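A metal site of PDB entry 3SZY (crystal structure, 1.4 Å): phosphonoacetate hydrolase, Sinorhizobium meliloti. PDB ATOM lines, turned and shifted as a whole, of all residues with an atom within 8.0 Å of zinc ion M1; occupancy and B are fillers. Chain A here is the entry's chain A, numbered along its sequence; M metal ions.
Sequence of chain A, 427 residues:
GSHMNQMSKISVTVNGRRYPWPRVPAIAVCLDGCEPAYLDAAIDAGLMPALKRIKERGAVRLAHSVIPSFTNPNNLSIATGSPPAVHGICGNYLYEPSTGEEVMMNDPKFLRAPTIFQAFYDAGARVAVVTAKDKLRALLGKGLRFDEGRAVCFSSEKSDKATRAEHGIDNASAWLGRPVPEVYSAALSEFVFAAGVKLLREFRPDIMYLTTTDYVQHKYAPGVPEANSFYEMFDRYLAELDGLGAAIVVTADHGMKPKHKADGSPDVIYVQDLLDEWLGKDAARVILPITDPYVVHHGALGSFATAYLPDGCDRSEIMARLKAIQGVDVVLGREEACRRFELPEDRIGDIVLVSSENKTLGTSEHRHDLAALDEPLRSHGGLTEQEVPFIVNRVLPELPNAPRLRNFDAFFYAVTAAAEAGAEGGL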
ATOM      1  N   ASP A  32     -13.838  -6.334  29.555  1.00  0.00           N
ATOM      2  CA  ASP A  32     -13.203  -5.298  28.756  1.00  0.00           C
ATOM      3  C   ASP A  32     -12.132  -4.539  29.551  1.00  0.00           C
ATOM      4  O   ASP A  32     -12.407  -4.053  30.651  1.00  0.00           O
ATOM      5  CB  ASP A  32     -14.279  -4.347  28.242  1.00  0.00           C
ATOM      6  CG  ASP A  32     -13.833  -3.574  27.036  1.00  0.00           C
ATOM      7  OD1 ASP A  32     -12.641  -3.199  26.961  1.00  0.00           O
ATOM      8  OD2 ASP A  32     -14.674  -3.318  26.152  1.00  0.00           O
ATOM      9  N   GLY A  33     -10.933  -4.451  28.991  1.00  0.00           N
ATOM     10  CA  GLY A  33      -9.835  -3.703  29.604  1.00  0.00           C
ATOM     11  C   GLY A  33      -9.307  -4.292  30.900  1.00  0.00           C
ATOM     12  O   GLY A  33      -8.613  -3.605  31.648  1.00  0.00           O
ATOM     13  N   SER A  69      -4.331  -3.873  20.403  1.00  0.00           N
ATOM     14  CA  SER A  69      -5.099  -4.280  21.580  1.00  0.00           C
ATOM     15  C   SER A  69      -6.274  -3.314  21.791  1.00  0.00           C
ATOM     16  O   SER A  69      -6.332  -2.595  22.787  1.00  0.00           O
ATOM     17  CB  SER A  69      -4.187  -4.440  22.814  1.00  0.00           C
ATOM     18  OG  SER A  69      -3.407  -3.293  23.078  1.00  0.00           O
ATOM     19  N   PHE A  70      -7.185  -3.349  20.823  1.00  0.00           N
ATOM     20  CA  PHE A  70      -8.388  -2.518  20.748  1.00  0.00           C
ATOM     21  C   PHE A  70      -9.624  -3.393  20.989  1.00  0.00           C
ATOM     22  O   PHE A  70      -9.585  -4.619  20.803  1.00  0.00           O
ATOM     23  CB  PHE A  70      -8.560  -1.914  19.342  1.00  0.00           C
ATOM     24  CG  PHE A  70      -7.535  -0.876  18.951  1.00  0.00           C
ATOM     25  CD1 PHE A  70      -6.783  -0.162  19.889  1.00  0.00           C
ATOM     26  CD2 PHE A  70      -7.382  -0.557  17.600  1.00  0.00           C
ATOM     27  CE1 PHE A  70      -5.863   0.809  19.465  1.00  0.00           C
ATOM     28  CE2 PHE A  70      -6.473   0.406  17.179  1.00  0.00           C
ATOM     29  CZ  PHE A  70      -5.715   1.088  18.107  1.00  0.00           C
ATOM     30  N   THR A  71     -10.731  -2.744  21.351  1.00  0.00           N
ATOM     31  CA  THR A  71     -11.980  -3.431  21.701  1.00  0.00           C
ATOM     32  C   THR A  71     -12.601  -4.253  20.569  1.00  0.00           C
ATOM     33  O   THR A  71     -12.798  -5.458  20.720  1.00  0.00           O
ATOM     34  CB  THR A  71     -13.002  -2.414  22.264  1.00  0.00           C
ATOM     35  OG1 THR A  71     -12.462  -1.835  23.466  1.00  0.00           O
ATOM     36  CG2 THR A  71     -14.330  -3.070  22.580  1.00  0.00           C
ATOM     37  N   THR A 213     -17.874  -3.113  28.858  1.00  0.00           N
ATOM     38  CA  THR A 213     -17.079  -1.967  28.386  1.00  0.00           C
ATOM     39  C   THR A 213     -15.944  -1.682  29.360  1.00  0.00           C
ATOM     40  O   THR A 213     -15.988  -2.128  30.514  1.00  0.00           O
ATOM     41  CB  THR A 213     -17.877  -0.642  28.189  1.00  0.00           C
ATOM     42  OG1 THR A 213     -18.038   0.027  29.449  1.00  0.00           O
ATOM     43  CG2 THR A 213     -19.212  -0.869  27.520  1.00  0.00           C
ATOM     44  N   ASP A 214     -14.954  -0.948  28.866  1.00  0.00           N
ATOM     45  CA  ASP A 214     -13.762  -0.578  29.627  1.00  0.00           C
ATOM     46  C   ASP A 214     -13.891   0.781  30.334  1.00  0.00           C
ATOM     47  O   ASP A 214     -12.875   1.417  30.643  1.00  0.00           O
ATOM     48  CB  ASP A 214     -12.490  -0.643  28.735  1.00  0.00           C
ATOM     49  CG  ASP A 214     -12.561   0.265  27.488  1.00  0.00           C
ATOM     50  OD1 ASP A 214     -13.603   0.910  27.277  1.00  0.00           O
ATOM     51  OD2 ASP A 214     -11.561   0.351  26.709  1.00  0.00           O
ATOM     52  N   TYR A 215     -15.117   1.221  30.601  1.00  0.00           N
ATOM     53  CA  TYR A 215     -15.370   2.523  31.238  1.00  0.00           C
ATOM     54  C   TYR A 215     -14.629   2.697  32.563  1.00  0.00           C
ATOM     55  O   TYR A 215     -13.882   3.670  32.739  1.00  0.00           O
ATOM     56  CB  TYR A 215     -16.871   2.763  31.447  1.00  0.00           C
ATOM     57  CG  TYR A 215     -17.168   3.969  32.307  1.00  0.00           C
ATOM     58  CD1 TYR A 215     -17.087   5.260  31.789  1.00  0.00           C
ATOM     59  CD2 TYR A 215     -17.494   3.829  33.662  1.00  0.00           C
ATOM     60  CE1 TYR A 215     -17.354   6.381  32.583  1.00  0.00           C
ATOM     61  CE2 TYR A 215     -17.750   4.940  34.463  1.00  0.00           C
ATOM     62  CZ  TYR A 215     -17.689   6.200  33.911  1.00  0.00           C
ATOM     63  OH  TYR A 215     -17.938   7.309  34.700  1.00  0.00           O
ATOM     64  N   GLN A 217     -12.241   0.933  33.764  1.00  0.00           N
ATOM     65  CA  GLN A 217     -10.821   0.630  33.619  1.00  0.00           C
ATOM     66  C   GLN A 217     -10.013   1.789  33.030  1.00  0.00           C
ATOM     67  O   GLN A 217      -8.861   2.010  33.414  1.00  0.00           O
ATOM     68  CB  GLN A 217     -10.653  -0.667  32.806  1.00  0.00           C
ATOM     69  CG  GLN A 217     -11.255  -1.924  33.462  1.00  0.00           C
ATOM     70  CD  GLN A 217     -12.781  -1.941  33.513  1.00  0.00           C
ATOM     71  OE1 GLN A 217     -13.463  -1.339  32.678  1.00  0.00           O
ATOM     72  NE2 GLN A 217     -13.339  -2.640  34.496  1.00  0.00           N
ATOM     73  N   HIS A 218     -10.621   2.553  32.118  1.00  0.00           N
ATOM     74  CA  HIS A 218     -10.010   3.798  31.625  1.00  0.00           C
ATOM     75  C   HIS A 218      -9.896   4.845  32.729  1.00  0.00           C
ATOM     76  O   HIS A 218      -9.016   5.699  32.680  1.00  0.00           O
ATOM     77  CB  HIS A 218     -10.805   4.397  30.457  1.00  0.00           C
ATOM     78  CG  HIS A 218     -10.450   3.844  29.113  1.00  0.00           C
ATOM     79  ND1 HIS A 218      -9.305   4.188  28.432  1.00  0.00           N
ATOM     80  CD2 HIS A 218     -11.130   2.992  28.297  1.00  0.00           C
ATOM     81  CE1 HIS A 218      -9.273   3.561  27.264  1.00  0.00           C
ATOM     82  NE2 HIS A 218     -10.367   2.830  27.165  1.00  0.00           N
ATOM     83  N   ASP A 253     -10.566  -8.554  26.214  1.00  0.00           N
ATOM     84  CA  ASP A 253     -10.195  -8.095  24.875  1.00  0.00           C
ATOM     85  C   ASP A 253      -8.790  -7.478  24.840  1.00  0.00           C
ATOM     86  O   ASP A 253      -8.085  -7.620  23.845  1.00  0.00           O
ATOM     87  CB  ASP A 253     -11.255  -7.138  24.294  1.00  0.00           C
ATOM     88  CG  ASP A 253     -11.590  -5.957  25.216  1.00  0.00           C
ATOM     89  OD1 ASP A 253     -11.126  -5.908  26.377  1.00  0.00           O
ATOM     90  OD2 ASP A 253     -12.339  -5.071  24.746  1.00  0.00           O
ATOM     91  N   HIS A 254      -8.397  -6.837  25.932  1.00  0.00           N
ATOM     92  CA  HIS A 254      -7.091  -6.196  26.075  1.00  0.00           C
ATOM     93  C   HIS A 254      -6.942  -5.753  27.526  1.00  0.00           C
ATOM     94  O   HIS A 254      -7.922  -5.731  28.274  1.00  0.00           O
ATOM     95  CB  HIS A 254      -6.965  -4.968  25.168  1.00  0.00           C
ATOM     96  CG  HIS A 254      -8.106  -4.009  25.309  1.00  0.00           C
ATOM     97  ND1 HIS A 254      -8.202  -3.124  26.358  1.00  0.00           N
ATOM     98  CD2 HIS A 254      -9.226  -3.830  24.569  1.00  0.00           C
ATOM     99  CE1 HIS A 254      -9.319  -2.430  26.246  1.00  0.00           C
ATOM    100  NE2 HIS A 254      -9.961  -2.846  25.175  1.00  0.00           N
ATOM    101  N   GLY A 255      -5.722  -5.376  27.897  1.00  0.00           N
ATOM    102  CA  GLY A 255      -5.442  -4.807  29.217  1.00  0.00           C
ATOM    103  C   GLY A 255      -5.584  -3.294  29.241  1.00  0.00           C
ATOM    104  O   GLY A 255      -6.330  -2.707  28.443  1.00  0.00           O
ATOM    105  N   MET A 256      -4.872  -2.659  30.161  1.00  0.00           N
ATOM    106  CA  MET A 256      -4.980  -1.217  30.386  1.00  0.00           C
ATOM    107  C   MET A 256      -3.733  -0.770  31.139  1.00  0.00           C
ATOM    108  O   MET A 256      -3.307  -1.442  32.083  1.00  0.00           O
ATOM    109  CB  MET A 256      -6.234  -0.896  31.200  1.00  0.00           C
ATOM    110  CG  MET A 256      -6.611   0.590  31.242  1.00  0.00           C
ATOM    111  SD  MET A 256      -7.288   1.223  29.704  1.00  0.00           S
ATOM    112  CE  MET A 256      -8.836   0.317  29.611  1.00  0.00           C
ATOM    113  N   ILE A 290      -8.348   3.379  17.491  1.00  0.00           N
ATOM    114  CA  ILE A 290      -8.839   2.986  18.826  1.00  0.00           C
ATOM    115  C   ILE A 290     -10.315   3.345  19.024  1.00  0.00           C
ATOM    116  O   ILE A 290     -11.029   2.650  19.746  1.00  0.00           O
ATOM    117  CB  ILE A 290      -7.977   3.576  19.989  1.00  0.00           C
ATOM    118  CG1 ILE A 290      -8.383   2.928  21.324  1.00  0.00           C
ATOM    119  CG2 ILE A 290      -8.060   5.118  20.039  1.00  0.00           C
ATOM    120  CD1 ILE A 290      -7.409   3.150  22.454  1.00  0.00           C
ATOM    121  N   THR A 291     -10.749   4.426  18.396  1.00  0.00           N
ATOM    122  CA  THR A 291     -12.145   4.855  18.478  1.00  0.00           C
ATOM    123  C   THR A 291     -12.591   5.447  17.141  1.00  0.00           C
ATOM    124  O   THR A 291     -11.856   5.405  16.155  1.00  0.00           O
ATOM    125  CB  THR A 291     -12.367   5.854  19.657  1.00  0.00           C
ATOM    126  OG1 THR A 291     -13.768   6.029  19.874  1.00  0.00           O
ATOM    127  CG2 THR A 291     -11.720   7.208  19.367  1.00  0.00           C
ATOM    128  N   GLY A 299     -10.239  10.313  24.387  1.00  0.00           N
ATOM    129  CA  GLY A 299     -10.682   8.956  24.079  1.00  0.00           C
ATOM    130  C   GLY A 299     -10.074   8.413  22.796  1.00  0.00           C
ATOM    131  O   GLY A 299     -10.044   7.205  22.570  1.00  0.00           O
ATOM    132  N   LEU A 301      -6.990   8.607  22.154  1.00  0.00           N
ATOM    133  CA  LEU A 301      -5.588   8.350  22.465  1.00  0.00           C
ATOM    134  C   LEU A 301      -5.332   6.916  22.884  1.00  0.00           C
ATOM    135  O   LEU A 301      -5.745   6.475  23.964  1.00  0.00           O
ATOM    136  CB  LEU A 301      -5.077   9.334  23.524  1.00  0.00           C
ATOM    137  CG  LEU A 301      -5.110  10.820  23.161  1.00  0.00           C
ATOM    138  CD1 LEU A 301      -4.747  11.669  24.366  1.00  0.00           C
ATOM    139  CD2 LEU A 301      -4.186  11.128  21.969  1.00  0.00           C
ATOM    140  N   ARG A 378      -5.558   6.783  31.052  1.00  0.00           N
ATOM    141  CA  ARG A 378      -5.256   5.359  30.985  1.00  0.00           C
ATOM    142  C   ARG A 378      -5.774   4.871  29.639  1.00  0.00           C
ATOM    143  O   ARG A 378      -6.846   5.294  29.197  1.00  0.00           O
ATOM    144  CB  ARG A 378      -5.946   4.595  32.117  1.00  0.00           C
ATOM    145  CG  ARG A 378      -5.549   5.042  33.526  1.00  0.00           C
ATOM    146  CD  ARG A 378      -6.362   4.331  34.603  1.00  0.00           C
ATOM    147  NE  ARG A 378      -6.333   2.879  34.481  1.00  0.00           N
ATOM    148  CZ  ARG A 378      -5.274   2.106  34.755  1.00  0.00           C
ATOM    149  NH1 ARG A 378      -4.143   2.642  35.184  1.00  0.00           N
ATOM    150  NH2 ARG A 378      -5.359   0.798  34.594  1.00  0.00           N
ATOM    151  N   SER A 379      -5.018   4.002  28.961  1.00  0.00           N
ATOM    152  CA  SER A 379      -5.472   3.494  27.672  1.00  0.00           C
ATOM    153  C   SER A 379      -4.810   2.184  27.273  1.00  0.00           C
ATOM    154  O   SER A 379      -4.158   1.523  28.087  1.00  0.00           O
ATOM    155  CB  SER A 379      -5.323   4.549  26.569  1.00  0.00           C
ATOM    156  OG  SER A 379      -6.188   4.274  25.476  1.00  0.00           O
ATOM    157  N   HIS A 380      -4.982   1.823  26.000  1.00  0.00           N
ATOM    158  CA  HIS A 380      -4.584   0.521  25.491  1.00  0.00           C
ATOM    159  C   HIS A 380      -4.282   0.634  24.008  1.00  0.00           C
ATOM    160  O   HIS A 380      -4.239   1.746  23.467  1.00  0.00           O
ATOM    161  CB  HIS A 380      -5.689  -0.520  25.768  1.00  0.00           C
ATOM    162  CG  HIS A 380      -7.056  -0.091  25.338  1.00  0.00           C
ATOM    163  ND1 HIS A 380      -7.624  -0.487  24.145  1.00  0.00           N
ATOM    164  CD2 HIS A 380      -7.969   0.712  25.944  1.00  0.00           C
ATOM    165  CE1 HIS A 380      -8.824   0.051  24.029  1.00  0.00           C
ATOM    166  NE2 HIS A 380      -9.057   0.784  25.109  1.00  0.00           N
ATOM    167  N   GLY A 381      -4.044  -0.497  23.347  1.00  0.00           N
ATOM    168  CA  GLY A 381      -3.737  -0.521  21.920  1.00  0.00           C
ATOM    169  C   GLY A 381      -2.375  -1.111  21.616  1.00  0.00           C
ATOM    170  O   GLY A 381      -2.170  -1.681  20.547  1.00  0.00           O
HETATM  171 ZN    ZN M   1     -10.957   1.684  25.451  1.00  0.00          ZN
HETATM  172 ZN    ZN M   2     -11.960  -2.799  25.217  1.00  0.00          ZN
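The backbone carbonyl oxygen of Arg 378 sits at hydrogen-bond distance from a ring nitrogen (ND1) of His 218 (2.8 Å).
A ring nitrogen (ND1) of His 254 sits close to a ring nitrogen (ND1) of His 380 (3.5 Å).
O of Ser 69 is in hydrogen-bond range of ND1 of His 380 (2.8 Å).
O of Asp 214 lies close to OE1 of Gln 217, 3.5 Å away.
Of the 22 residues printed, 3 come within 4 Å of zinc ion M1.
Zinc ion M1 is bound by the side-chain carboxylate of Asp 214, a ring nitrogen (NE2) of His 380 and a ring nitrogen (NE2) of His 218.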
